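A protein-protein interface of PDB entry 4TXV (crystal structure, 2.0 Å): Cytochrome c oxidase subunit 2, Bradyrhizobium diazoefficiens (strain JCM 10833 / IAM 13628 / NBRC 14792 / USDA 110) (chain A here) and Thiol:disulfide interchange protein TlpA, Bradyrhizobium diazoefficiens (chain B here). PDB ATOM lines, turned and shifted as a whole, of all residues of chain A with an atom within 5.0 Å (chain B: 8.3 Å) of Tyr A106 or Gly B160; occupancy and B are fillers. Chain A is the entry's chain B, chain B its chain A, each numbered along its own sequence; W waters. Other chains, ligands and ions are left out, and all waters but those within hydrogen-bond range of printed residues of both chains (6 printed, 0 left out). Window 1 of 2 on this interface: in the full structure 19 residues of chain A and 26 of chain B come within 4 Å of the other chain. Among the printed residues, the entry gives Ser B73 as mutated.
Water W5 lies within hydrogen-bond range of the side-chain carboxylate (OE2) of Glu B163 (2.6 Å), the guanidinium group (NE) of Arg A47 (2.9 Å) and the backbone carbonyl oxygen (O) of Leu A49 (3.3 Å). Water W3 bridges the side-chain hydroxyl of Tyr A106 (2.6 Å) and the side-chain carboxylate of Glu B25 (2.8 Å). Water W4 lies within hydrogen-bond range of the backbone carbonyl oxygen of Met A104 (2.7 Å), the backbone carbonyl oxygen of Glu B25 (2.9 Å), the backbone NH of Ala B28 (3.2 Å) and the backbone NH of Ala B27 (3.4 Å). Water W2 bridges the side-chain amino group of Lys B75 (2.7 Å) and the backbone carbonyl oxygen of Gly A50 (3.2 Å). Water W1 lies within hydrogen-bond range of O of Pro B161 (2.8 Å) and N of Tyr A106 (3.1 Å). Water W6 lies within hydrogen-bond range of the backbone NH (N) of Leu B140, the side-chain hydroxyl (OG1) of Thr B144 and the side-chain amide nitrogen (NE2) of Gln A108.
The backbone carbonyl oxygen of Thr B144 lies within hydrogen-bond range of the backbone NH of Leu B65 (2.9 Å). The side-chain sulfur of Cys B70 sits at hydrogen-bond distance from the backbone carbonyl oxygen of Met B142. The side-chain carboxylate (OE1) of Glu B76 lies within hydrogen-bond range of the backbone NH (N) of Ala B162. O of Gly B141 is in hydrogen-bond range of OG1 of Thr B144 (2.7 Å). O of Pro B143 is in hydrogen-bond range of N of Gly B160. O of Ile A122 lies within hydrogen-bond range of N of Gly A107, at 3.0 Å.
Printed residues of chain B that touch a printed residue of chain A: Gly B24, Glu B25, Ala B27, Ala B28, Lys B75, Leu B140, Gly B141, Met B142, Pro B143, Thr B144, Ala B159, Gly B160, Pro B161, Ala B162 and Glu B163.
Lys B75 touches Leu A49. Leu A49 touches Pro B161 (CD1 to CB, 3.97 Å). Ala B162 touches Leu A49 (C to CD1, 3.5 Å). Ala B27 touches Met A104 (CB to O, 3.8 Å). CB of Ala B27 touches CZ of Phe A105, 3.5 Å away. Tyr A106 touches Gly B160 (O to CA, 3.96 Å). Tyr A106 touches Pro B161. Gln A108 touches Leu B140. CA of Gln A108 touches O of Met B142, 3.4 Å away. NE2 of Gln A108 touches C of Ala B159 (3.2 Å).
Of the printed residues of chain B, Met A104 touches Gly B24 (3.1 Å), Glu B25 (3.8 Å) and Ala B27 (3.8 Å). Of the printed residues of chain A, Glu B25 touches Met A104. Of the printed residues of chain A, Ala B27 touches Met A104 (3.8 Å) and Phe A105 (3.5 Å). Of the printed residues of chain A, Ala B159 touches Gln A108 (3.2 Å). Of the printed residues of chain A, Ala B162 touches Leu A49. The nearest residue of chain A that does not touch Gly B160 is Gly A107 (4.5 Å). The nearest printed residue of chain A that does not touch Glu B25 is Tyr A106 (4.5 Å).
The backbone carbonyl oxygen of Gly B24 lies within hydrogen-bond range of the backbone NH of Met A104. The side-chain amide nitrogen of Gln A108 is in hydrogen-bond range of the backbone carbonyl oxygen of Gly B141 (3.3 Å). O of Pro B143 is in hydrogen-bond range of NE2 of Gln A108 (2.8 Å). The backbone NH (N) of Leu A49 lies within hydrogen-bond range of the side-chain carboxylate (OE2) of Glu B163 (3.0 Å).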
ATOM      1  N   ARG A  47      -9.396   8.185   2.318  1.00  0.00           N
ATOM      2  CA  ARG A  47     -10.588   7.793   3.113  1.00  0.00           C
ATOM      3  C   ARG A  47     -10.651   6.354   3.451  1.00  0.00           C
ATOM      4  O   ARG A  47     -10.224   5.513   2.677  1.00  0.00           O
ATOM      5  CB  ARG A  47     -11.871   8.114   2.404  1.00  0.00           C
ATOM      6  CG  ARG A  47     -11.993   9.601   2.091  1.00  0.00           C
ATOM      7  CD  ARG A  47     -13.285   9.857   1.347  1.00  0.00           C
ATOM      8  NE  ARG A  47     -14.454   9.287   2.044  1.00  0.00           N
ATOM      9  CZ  ARG A  47     -15.676   9.332   1.547  1.00  0.00           C
ATOM     10  NH1 ARG A  47     -15.898   9.966   0.403  1.00  0.00           N
ATOM     11  NH2 ARG A  47     -16.691   8.788   2.224  1.00  0.00           N
ATOM     12  N   LEU A  49     -13.692   5.186   5.357  1.00  0.00           N
ATOM     13  CA  LEU A  49     -15.145   4.866   5.503  1.00  0.00           C
ATOM     14  C   LEU A  49     -15.944   5.498   4.399  1.00  0.00           C
ATOM     15  O   LEU A  49     -15.545   6.512   3.877  1.00  0.00           O
ATOM     16  CB  LEU A  49     -15.662   5.447   6.760  1.00  0.00           C
ATOM     17  CG  LEU A  49     -14.941   4.956   7.992  1.00  0.00           C
ATOM     18  CD1 LEU A  49     -15.506   5.712   9.165  1.00  0.00           C
ATOM     19  CD2 LEU A  49     -15.163   3.448   8.123  1.00  0.00           C
ATOM     20  N   GLY A  50     -17.088   4.905   4.092  1.00  0.00           N
ATOM     21  CA  GLY A  50     -18.175   5.669   3.514  1.00  0.00           C
ATOM     22  C   GLY A  50     -18.648   5.133   2.213  1.00  0.00           C
ATOM     23  O   GLY A  50     -18.249   4.071   1.815  1.00  0.00           O
ATOM     24  N   VAL A  51     -19.476   5.909   1.553  1.00  0.00           N
ATOM     25  CA  VAL A  51     -20.208   5.471   0.383  1.00  0.00           C
ATOM     26  C   VAL A  51     -19.969   6.503  -0.714  1.00  0.00           C
ATOM     27  O   VAL A  51     -19.424   7.562  -0.426  1.00  0.00           O
ATOM     28  CB  VAL A  51     -21.697   5.429   0.671  1.00  0.00           C
ATOM     29  CG1 VAL A  51     -22.036   4.427   1.772  1.00  0.00           C
ATOM     30  CG2 VAL A  51     -22.191   6.820   1.031  1.00  0.00           C
ATOM     31  N   GLU A  54     -24.226   9.845  -0.311  1.00  0.00           N
ATOM     32  CA  GLU A  54     -24.701   9.832   1.048  1.00  0.00           C
ATOM     33  C   GLU A  54     -26.126  10.282   1.085  1.00  0.00           C
ATOM     34  O   GLU A  54     -26.568  11.064   0.229  1.00  0.00           O
ATOM     35  CB  GLU A  54     -23.907  10.795   1.930  1.00  0.00           C
ATOM     36  CG  GLU A  54     -22.500  10.313   2.276  1.00  0.00           C
ATOM     37  CD  GLU A  54     -21.407  11.071   1.544  1.00  0.00           C
ATOM     38  OE1 GLU A  54     -21.767  11.820   0.607  1.00  0.00           O
ATOM     39  OE2 GLU A  54     -20.215  10.879   1.890  1.00  0.00           O
ATOM     40  N   LEU A  78     -29.821   4.022  12.940  1.00  0.00           N
ATOM     41  CA  LEU A  78     -28.807   5.036  13.136  1.00  0.00           C
ATOM     42  C   LEU A  78     -29.008   5.518  14.571  1.00  0.00           C
ATOM     43  O   LEU A  78     -29.823   6.426  14.838  1.00  0.00           O
ATOM     44  CB  LEU A  78     -28.937   6.181  12.086  1.00  0.00           C
ATOM     45  CG  LEU A  78     -27.692   7.044  11.834  1.00  0.00           C
ATOM     46  CD1 LEU A  78     -27.091   7.566  13.159  1.00  0.00           C
ATOM     47  CD2 LEU A  78     -26.650   6.263  11.052  1.00  0.00           C
ATOM     48  N   MET A 104     -20.952  13.758   9.547  1.00  0.00           N
ATOM     49  CA  MET A 104     -21.188  12.426   9.044  1.00  0.00           C
ATOM     50  C   MET A 104     -21.646  11.474  10.120  1.00  0.00           C
ATOM     51  O   MET A 104     -21.163  11.499  11.288  1.00  0.00           O
ATOM     52  CB  MET A 104     -19.914  11.877   8.425  1.00  0.00           C
ATOM     53  CG  MET A 104     -19.475  12.647   7.192  1.00  0.00           C
ATOM     54  SD  MET A 104     -20.695  12.634   5.827  1.00  0.00           S
ATOM     55  CE  MET A 104     -21.263  10.970   5.649  1.00  0.00           C
ATOM     56  N   PHE A 105     -22.596  10.649   9.728  1.00  0.00           N
ATOM     57  CA  PHE A 105     -23.172   9.606  10.624  1.00  0.00           C
ATOM     58  C   PHE A 105     -23.234   8.271   9.902  1.00  0.00           C
ATOM     59  O   PHE A 105     -23.893   8.126   8.899  1.00  0.00           O
ATOM     60  CB  PHE A 105     -24.557   9.996  11.111  1.00  0.00           C
ATOM     61  CG  PHE A 105     -24.594  11.295  11.891  1.00  0.00           C
ATOM     62  CD1 PHE A 105     -24.567  12.537  11.261  1.00  0.00           C
ATOM     63  CD2 PHE A 105     -24.703  11.263  13.256  1.00  0.00           C
ATOM     64  CE1 PHE A 105     -24.581  13.727  12.007  1.00  0.00           C
ATOM     65  CE2 PHE A 105     -24.761  12.446  13.996  1.00  0.00           C
ATOM     66  CZ  PHE A 105     -24.712  13.671  13.384  1.00  0.00           C
ATOM     67  N   TYR A 106     -22.485   7.301  10.424  1.00  0.00           N
ATOM     68  CA  TYR A 106     -22.434   5.976   9.877  1.00  0.00           C
ATOM     69  C   TYR A 106     -23.113   4.937  10.771  1.00  0.00           C
ATOM     70  O   TYR A 106     -22.985   4.923  12.020  1.00  0.00           O
ATOM     71  CB  TYR A 106     -20.988   5.597   9.649  1.00  0.00           C
ATOM     72  CG  TYR A 106     -20.316   6.437   8.559  1.00  0.00           C
ATOM     73  CD1 TYR A 106     -20.731   6.364   7.259  1.00  0.00           C
ATOM     74  CD2 TYR A 106     -19.212   7.245   8.836  1.00  0.00           C
ATOM     75  CE1 TYR A 106     -20.072   7.071   6.254  1.00  0.00           C
ATOM     76  CE2 TYR A 106     -18.549   7.961   7.830  1.00  0.00           C
ATOM     77  CZ  TYR A 106     -19.006   7.868   6.531  1.00  0.00           C
ATOM     78  OH  TYR A 106     -18.402   8.594   5.504  1.00  0.00           O
ATOM     79  N   GLY A 107     -23.734   3.969  10.119  1.00  0.00           N
ATOM     80  CA  GLY A 107     -24.401   2.874  10.873  1.00  0.00           C
ATOM     81  C   GLY A 107     -23.459   1.800  11.413  1.00  0.00           C
ATOM     82  O   GLY A 107     -22.236   1.787  11.137  1.00  0.00           O
ATOM     83  N   GLN A 108     -24.049   0.860  12.145  1.00  0.00           N
ATOM     84  CA  GLN A 108     -23.333  -0.232  12.763  1.00  0.00           C
ATOM     85  C   GLN A 108     -23.653  -1.578  12.157  1.00  0.00           C
ATOM     86  O   GLN A 108     -24.679  -1.716  11.528  1.00  0.00           O
ATOM     87  CB  GLN A 108     -23.737  -0.288  14.218  1.00  0.00           C
ATOM     88  CG  GLN A 108     -23.122   0.804  15.033  1.00  0.00           C
ATOM     89  CD  GLN A 108     -23.558   0.714  16.477  1.00  0.00           C
ATOM     90  OE1 GLN A 108     -24.772   0.622  16.785  1.00  0.00           O
ATOM     91  NE2 GLN A 108     -22.607   0.720  17.370  1.00  0.00           N
ATOM     92  N   ILE A 122     -25.032   2.525   5.894  1.00  0.00           N
ATOM     93  CA  ILE A 122     -25.836   3.720   6.040  1.00  0.00           C
ATOM     94  C   ILE A 122     -24.939   4.911   6.317  1.00  0.00           C
ATOM     95  O   ILE A 122     -24.179   4.908   7.308  1.00  0.00           O
ATOM     96  CB  ILE A 122     -26.859   3.539   7.214  1.00  0.00           C
ATOM     97  CG1 ILE A 122     -27.738   2.362   6.872  1.00  0.00           C
ATOM     98  CG2 ILE A 122     -27.731   4.769   7.345  1.00  0.00           C
ATOM     99  CD1 ILE A 122     -28.814   2.013   7.864  1.00  0.00           C
ATOM    100  N   ALA A 123     -25.064   5.945   5.473  1.00  0.00           N
ATOM    101  CA  ALA A 123     -24.268   7.117   5.590  1.00  0.00           C
ATOM    102  C   ALA A 123     -25.117   8.341   5.418  1.00  0.00           C
ATOM    103  O   ALA A 123     -25.647   8.656   4.323  1.00  0.00           O
ATOM    104  CB  ALA A 123     -23.139   7.119   4.561  1.00  0.00           C
ATOM    105  N   GLY B  24     -18.698  17.153  12.347  1.00  0.00           N
ATOM    106  CA  GLY B  24     -17.972  16.681  11.177  1.00  0.00           C
ATOM    107  C   GLY B  24     -17.797  15.182  11.244  1.00  0.00           C
ATOM    108  O   GLY B  24     -18.721  14.436  11.536  1.00  0.00           O
ATOM    109  N   GLU B  25     -16.579  14.721  11.055  1.00  0.00           N
ATOM    110  CA  GLU B  25     -16.345  13.267  10.954  1.00  0.00           C
ATOM    111  C   GLU B  25     -16.685  12.557  12.301  1.00  0.00           C
ATOM    112  O   GLU B  25     -16.930  11.332  12.301  1.00  0.00           O
ATOM    113  CB  GLU B  25     -14.894  12.996  10.511  1.00  0.00           C
ATOM    114  CG  GLU B  25     -14.580  13.477   9.085  1.00  0.00           C
ATOM    115  CD  GLU B  25     -15.399  12.771   7.997  1.00  0.00           C
ATOM    116  OE1 GLU B  25     -15.947  11.652   8.291  1.00  0.00           O
ATOM    117  OE2 GLU B  25     -15.467  13.330   6.836  1.00  0.00           O
ATOM    118  N   VAL B  26     -16.729  13.328  13.408  1.00  0.00           N
ATOM    119  CA  VAL B  26     -17.066  12.751  14.708  1.00  0.00           C
ATOM    120  C   VAL B  26     -18.421  13.256  15.295  1.00  0.00           C
ATOM    121  O   VAL B  26     -18.622  13.220  16.482  1.00  0.00           O
ATOM    122  CB  VAL B  26     -15.914  12.857  15.745  1.00  0.00           C
ATOM    123  CG1 VAL B  26     -14.745  11.999  15.291  1.00  0.00           C
ATOM    124  CG2 VAL B  26     -15.524  14.310  16.072  1.00  0.00           C
ATOM    125  N   ALA B  27     -19.366  13.597  14.407  1.00  0.00           N
ATOM    126  CA  ALA B  27     -20.630  14.150  14.791  1.00  0.00           C
ATOM    127  C   ALA B  27     -21.474  13.196  15.617  1.00  0.00           C
ATOM    128  O   ALA B  27     -22.251  13.631  16.455  1.00  0.00           O
ATOM    129  CB  ALA B  27     -21.384  14.601  13.549  1.00  0.00           C
ATOM    130  N   ALA B  28     -21.313  11.906  15.380  1.00  0.00           N
ATOM    131  CA  ALA B  28     -22.132  10.874  16.041  1.00  0.00           C
ATOM    132  C   ALA B  28     -21.716  10.596  17.512  1.00  0.00           C
ATOM    133  O   ALA B  28     -22.349   9.820  18.159  1.00  0.00           O
ATOM    134  CB  ALA B  28     -22.043   9.574  15.243  1.00  0.00           C
ATOM    135  N   LEU B  29     -20.664  11.209  18.001  1.00  0.00           N
ATOM    136  CA  LEU B  29     -20.335  11.128  19.404  1.00  0.00           C
ATOM    137  C   LEU B  29     -21.448  11.715  20.202  1.00  0.00           C
ATOM    138  O   LEU B  29     -22.011  12.754  19.811  1.00  0.00           O
ATOM    139  CB  LEU B  29     -19.100  11.914  19.681  1.00  0.00           C
ATOM    140  CG  LEU B  29     -17.812  11.183  19.512  1.00  0.00           C
ATOM    141  CD1 LEU B  29     -16.800  12.277  19.587  1.00  0.00           C
ATOM    142  CD2 LEU B  29     -17.530  10.063  20.554  1.00  0.00           C
ATOM    143  N   ASN B  64     -12.137   1.144  22.164  1.00  0.00           N
ATOM    144  CA  ASN B  64     -12.897   0.707  20.990  1.00  0.00           C
ATOM    145  C   ASN B  64     -13.086  -0.804  21.043  1.00  0.00           C
ATOM    146  O   ASN B  64     -12.185  -1.517  21.498  1.00  0.00           O
ATOM    147  CB  ASN B  64     -12.066   1.069  19.778  1.00  0.00           C
ATOM    148  CG  ASN B  64     -12.549   0.356  18.522  1.00  0.00           C
ATOM    149  OD1 ASN B  64     -11.944  -0.622  18.067  1.00  0.00           O
ATOM    150  ND2 ASN B  64     -13.669   0.812  17.995  1.00  0.00           N
ATOM    151  N   LEU B  65     -14.216  -1.317  20.578  1.00  0.00           N
ATOM    152  CA  LEU B  65     -14.419  -2.735  20.464  1.00  0.00           C
ATOM    153  C   LEU B  65     -14.510  -2.989  18.974  1.00  0.00           C
ATOM    154  O   LEU B  65     -15.256  -2.297  18.278  1.00  0.00           O
ATOM    155  CB  LEU B  65     -15.687  -3.188  21.099  1.00  0.00           C
ATOM    156  CG  LEU B  65     -15.957  -2.810  22.534  1.00  0.00           C
ATOM    157  CD1 LEU B  65     -17.178  -3.527  23.044  1.00  0.00           C
ATOM    158  CD2 LEU B  65     -14.769  -3.199  23.387  1.00  0.00           C
ATOM    159  N   CYS B  70     -16.975  -7.698  11.533  1.00  0.00           N
ATOM    160  CA  CYS B  70     -17.696  -6.421  11.349  1.00  0.00           C
ATOM    161  C   CYS B  70     -16.915  -5.486  10.439  1.00  0.00           C
ATOM    162  O   CYS B  70     -15.849  -4.982  10.810  1.00  0.00           O
ATOM    163  CB  CYS B  70     -17.933  -5.780  12.710  1.00  0.00           C
ATOM    164  SG  CYS B  70     -18.594  -4.110  12.592  1.00  0.00           S
ATOM    165  N   PRO B  72     -17.353  -2.228   9.141  1.00  0.00           N
ATOM    166  CA  PRO B  72     -16.983  -0.873   9.590  1.00  0.00           C
ATOM    167  C   PRO B  72     -15.949  -0.862  10.727  1.00  0.00           C
ATOM    168  O   PRO B  72     -15.113   0.017  10.765  1.00  0.00           O
ATOM    169  CB  PRO B  72     -18.332  -0.238  10.032  1.00  0.00           C
ATOM    170  CG  PRO B  72     -19.336  -1.342  10.068  1.00  0.00           C
ATOM    171  CD  PRO B  72     -18.818  -2.417   9.121  1.00  0.00           C
ATOM    172  N   SER B  73     -15.996  -1.846  11.615  1.00  0.00           N
ATOM    173  CA  SER B  73     -15.006  -1.920  12.678  1.00  0.00           C
ATOM    174  C   SER B  73     -13.607  -2.268  12.140  1.00  0.00           C
ATOM    175  O   SER B  73     -12.588  -1.716  12.638  1.00  0.00           O
ATOM    176  CB  SER B  73     -15.402  -2.885  13.762  1.00  0.00           C
ATOM    177  OG  SER B  73     -14.671  -4.052  13.678  1.00  0.00           O
ATOM    178  N   LYS B  75     -12.592  -1.470   9.034  1.00  0.00           N
ATOM    179  CA  LYS B  75     -12.214  -0.320   8.236  1.00  0.00           C
ATOM    180  C   LYS B  75     -11.626   0.842   8.980  1.00  0.00           C
ATOM    181  O   LYS B  75     -10.755   1.529   8.438  1.00  0.00           O
ATOM    182  CB  LYS B  75     -13.403   0.211   7.440  1.00  0.00           C
ATOM    183  CG  LYS B  75     -13.740  -0.610   6.214  1.00  0.00           C
ATOM    184  CD  LYS B  75     -14.989  -0.029   5.614  1.00  0.00           C
ATOM    185  CE  LYS B  75     -15.225  -0.356   4.159  1.00  0.00           C
ATOM    186  NZ  LYS B  75     -16.411   0.492   3.793  1.00  0.00           N
ATOM    187  N   GLU B  76     -12.085   1.100  10.182  1.00  0.00           N
ATOM    188  CA  GLU B  76     -11.602   2.275  10.910  1.00  0.00           C
ATOM    189  C   GLU B  76     -10.337   1.907  11.658  1.00  0.00           C
ATOM    190  O   GLU B  76      -9.745   2.768  12.314  1.00  0.00           O
ATOM    191  CB  GLU B  76     -12.654   2.827  11.910  1.00  0.00           C
ATOM    192  CG  GLU B  76     -12.909   1.919  13.101  1.00  0.00           C
ATOM    193  CD  GLU B  76     -13.923   2.493  14.085  1.00  0.00           C
ATOM    194  OE1 GLU B  76     -14.332   3.638  13.905  1.00  0.00           O
ATOM    195  OE2 GLU B  76     -14.285   1.800  15.064  1.00  0.00           O
ATOM    196  N   LEU B 140     -24.780  -0.912  21.390  1.00  0.00           N
ATOM    197  CA  LEU B 140     -25.919  -1.245  20.522  1.00  0.00           C
ATOM    198  C   LEU B 140     -25.501  -1.967  19.279  1.00  0.00           C
ATOM    199  O   LEU B 140     -26.335  -2.367  18.505  1.00  0.00           O
ATOM    200  CB  LEU B 140     -26.570   0.059  20.077  1.00  0.00           C
ATOM    201  CG  LEU B 140     -26.946   0.982  21.240  1.00  0.00           C
ATOM    202  CD1 LEU B 140     -27.429   2.326  20.720  1.00  0.00           C
ATOM    203  CD2 LEU B 140     -28.032   0.309  22.099  1.00  0.00           C
ATOM    204  N   GLY B 141     -24.203  -2.075  19.021  1.00  0.00           N
ATOM    205  CA  GLY B 141     -23.776  -2.659  17.774  1.00  0.00           C
ATOM    206  C   GLY B 141     -22.280  -2.600  17.691  1.00  0.00           C
ATOM    207  O   GLY B 141     -21.571  -2.194  18.634  1.00  0.00           O
ATOM    208  N   MET B 142     -21.786  -2.922  16.518  1.00  0.00           N
ATOM    209  CA  MET B 142     -20.374  -2.784  16.294  1.00  0.00           C
ATOM    210  C   MET B 142     -20.025  -1.918  15.096  1.00  0.00           C
ATOM    211  O   MET B 142     -20.709  -1.962  14.042  1.00  0.00           O
ATOM    212  CB  MET B 142     -19.825  -4.204  16.087  1.00  0.00           C
ATOM    213  CG  MET B 142     -19.751  -5.028  17.365  1.00  0.00           C
ATOM    214  SD  MET B 142     -18.537  -4.430  18.541  1.00  0.00           S
ATOM    215  CE  MET B 142     -17.001  -5.007  17.792  1.00  0.00           C
ATOM    216  N   PRO B 143     -18.908  -1.182  15.188  1.00  0.00           N
ATOM    217  CA  PRO B 143     -18.068  -0.998  16.373  1.00  0.00           C
ATOM    218  C   PRO B 143     -18.766  -0.075  17.373  1.00  0.00           C
ATOM    219  O   PRO B 143     -19.794   0.569  17.045  1.00  0.00           O
ATOM    220  CB  PRO B 143     -16.839  -0.265  15.815  1.00  0.00           C
ATOM    221  CG  PRO B 143     -17.404   0.560  14.678  1.00  0.00           C
ATOM    222  CD  PRO B 143     -18.472  -0.316  14.066  1.00  0.00           C
ATOM    223  N   THR B 144     -18.224  -0.063  18.577  1.00  0.00           N
ATOM    224  CA  THR B 144     -18.536   0.929  19.603  1.00  0.00           C
ATOM    225  C   THR B 144     -17.275   1.445  20.143  1.00  0.00           C
ATOM    226  O   THR B 144     -16.345   0.655  20.275  1.00  0.00           O
ATOM    227  CB  THR B 144     -19.233   0.259  20.791  1.00  0.00           C
ATOM    228  OG1 THR B 144     -20.387  -0.401  20.313  1.00  0.00           O
ATOM    229  CG2 THR B 144     -19.699   1.311  21.768  1.00  0.00           C
ATOM    230  N   SER B 145     -17.204   2.753  20.404  1.00  0.00           N
ATOM    231  CA  SER B 145     -16.079   3.355  21.064  1.00  0.00           C
ATOM    232  C   SER B 145     -16.534   4.287  22.170  1.00  0.00           C
ATOM    233  O   SER B 145     -17.534   5.002  22.054  1.00  0.00           O
ATOM    234  CB  SER B 145     -15.172   4.149  20.097  1.00  0.00           C
ATOM    235  OG  SER B 145     -14.864   3.389  18.927  1.00  0.00           O
ATOM    236  N   VAL B 146     -15.730   4.322  23.221  1.00  0.00           N
ATOM    237  CA  VAL B 146     -15.988   5.175  24.348  1.00  0.00           C
ATOM    238  C   VAL B 146     -14.757   5.991  24.693  1.00  0.00           C
ATOM    239  O   VAL B 146     -13.637   5.454  24.848  1.00  0.00           O
ATOM    240  CB  VAL B 146     -16.366   4.331  25.583  1.00  0.00           C
ATOM    241  CG1 VAL B 146     -16.802   5.233  26.732  1.00  0.00           C
ATOM    242  CG2 VAL B 146     -17.467   3.370  25.238  1.00  0.00           C
ATOM    243  N   THR B 157     -19.690   8.618  23.958  1.00  0.00           N
ATOM    244  CA  THR B 157     -19.732   7.322  23.326  1.00  0.00           C
ATOM    245  C   THR B 157     -20.206   7.518  21.927  1.00  0.00           C
ATOM    246  O   THR B 157     -21.097   8.365  21.695  1.00  0.00           O
ATOM    247  CB  THR B 157     -20.721   6.401  24.039  1.00  0.00           C
ATOM    248  OG1 THR B 157     -20.244   6.174  25.364  1.00  0.00           O
ATOM    249  CG2 THR B 157     -20.860   5.031  23.324  1.00  0.00           C
ATOM    250  N   ILE B 158     -19.640   6.717  21.020  1.00  0.00           N
ATOM    251  CA  ILE B 158     -20.111   6.648  19.641  1.00  0.00           C
ATOM    252  C   ILE B 158     -20.502   5.223  19.243  1.00  0.00           C
ATOM    253  O   ILE B 158     -19.710   4.274  19.404  1.00  0.00           O
ATOM    254  CB  ILE B 158     -19.105   7.253  18.643  1.00  0.00           C
ATOM    255  CG1 ILE B 158     -19.706   7.107  17.227  1.00  0.00           C
ATOM    256  CG2 ILE B 158     -17.751   6.499  18.624  1.00  0.00           C
ATOM    257  CD1 ILE B 158     -18.894   7.790  16.165  1.00  0.00           C
ATOM    258  N   ALA B 159     -21.743   5.088  18.777  1.00  0.00           N
ATOM    259  CA  ALA B 159     -22.309   3.829  18.298  1.00  0.00           C
ATOM    260  C   ALA B 159     -22.216   3.827  16.772  1.00  0.00           C
ATOM    261  O   ALA B 159     -23.207   3.972  16.033  1.00  0.00           O
ATOM    262  CB  ALA B 159     -23.762   3.620  18.807  1.00  0.00           C
ATOM    263  N   GLY B 160     -20.971   3.639  16.330  1.00  0.00           N
ATOM    264  CA  GLY B 160     -20.632   3.585  14.913  1.00  0.00           C
ATOM    265  C   GLY B 160     -19.163   3.812  14.698  1.00  0.00           C
ATOM    266  O   GLY B 160     -18.431   4.181  15.649  1.00  0.00           O
ATOM    267  N   PRO B 161     -18.721   3.678  13.436  1.00  0.00           N
ATOM    268  CA  PRO B 161     -17.355   3.998  13.059  1.00  0.00           C
ATOM    269  C   PRO B 161     -17.185   5.490  12.758  1.00  0.00           C
ATOM    270  O   PRO B 161     -18.173   6.199  12.496  1.00  0.00           O
ATOM    271  CB  PRO B 161     -17.229   3.276  11.777  1.00  0.00           C
ATOM    272  CG  PRO B 161     -18.556   3.444  11.099  1.00  0.00           C
ATOM    273  CD  PRO B 161     -19.558   3.424  12.243  1.00  0.00           C
ATOM    274  N   ALA B 162     -15.960   5.957  12.741  1.00  0.00           N
ATOM    275  CA  ALA B 162     -15.639   7.314  12.413  1.00  0.00           C
ATOM    276  C   ALA B 162     -14.205   7.383  11.928  1.00  0.00           C
ATOM    277  O   ALA B 162     -13.386   6.520  12.261  1.00  0.00           O
ATOM    278  CB  ALA B 162     -15.817   8.225  13.636  1.00  0.00           C
ATOM    279  N   GLU B 163     -13.920   8.420  11.142  1.00  0.00           N
ATOM    280  CA  GLU B 163     -12.551   8.797  10.717  1.00  0.00           C
ATOM    281  C   GLU B 163     -11.796   9.421  11.885  1.00  0.00           C
ATOM    282  O   GLU B 163     -11.709  10.626  12.060  1.00  0.00           O
ATOM    283  CB  GLU B 163     -12.611   9.724   9.523  1.00  0.00           C
ATOM    284  CG  GLU B 163     -13.198   9.102   8.251  1.00  0.00           C
ATOM    285  CD  GLU B 163     -12.201   8.256   7.446  1.00  0.00           C
ATOM    286  OE1 GLU B 163     -11.086   7.976   7.973  1.00  0.00           O
ATOM    287  OE2 GLU B 163     -12.574   7.838   6.297  1.00  0.00           O
ATOM    288  N   TRP B 164     -11.287   8.531  12.716  1.00  0.00           N
ATOM    289  CA  TRP B 164     -10.694   8.823  14.031  1.00  0.00           C
ATOM    290  C   TRP B 164      -9.312   9.463  13.926  1.00  0.00           C
ATOM    291  O   TRP B 164      -8.749   9.932  14.972  1.00  0.00           O
ATOM    292  CB  TRP B 164     -10.621   7.511  14.872  1.00  0.00           C
ATOM    293  CG  TRP B 164     -11.911   7.231  15.592  1.00  0.00           C
ATOM    294  CD1 TRP B 164     -12.825   6.210  15.393  1.00  0.00           C
ATOM    295  CD2 TRP B 164     -12.439   8.032  16.623  1.00  0.00           C
ATOM    296  NE1 TRP B 164     -13.885   6.353  16.298  1.00  0.00           N
ATOM    297  CE2 TRP B 164     -13.674   7.479  17.024  1.00  0.00           C
ATOM    298  CE3 TRP B 164     -11.994   9.189  17.237  1.00  0.00           C
ATOM    299  CZ2 TRP B 164     -14.407   8.021  18.032  1.00  0.00           C
ATOM    300  CZ3 TRP B 164     -12.745   9.734  18.229  1.00  0.00           C
ATOM    301  CH2 TRP B 164     -13.937   9.153  18.600  1.00  0.00           C
HETATM  302  O   HOH W   1     -20.492   7.785  12.715  1.00  0.00           O
HETATM  303  O   HOH W   2     -15.464   2.499   2.237  1.00  0.00           O
HETATM  304  O   HOH W   3     -16.493  10.271   5.896  1.00  0.00           O
HETATM  305  O   HOH W   4     -19.532  10.456  13.137  1.00  0.00           O
HETATM  306  O   HOH W   5     -14.144   9.317   4.915  1.00  0.00           O
HETATM  307  O   HOH W   6     -22.948   1.093  20.408  1.00  0.00           O
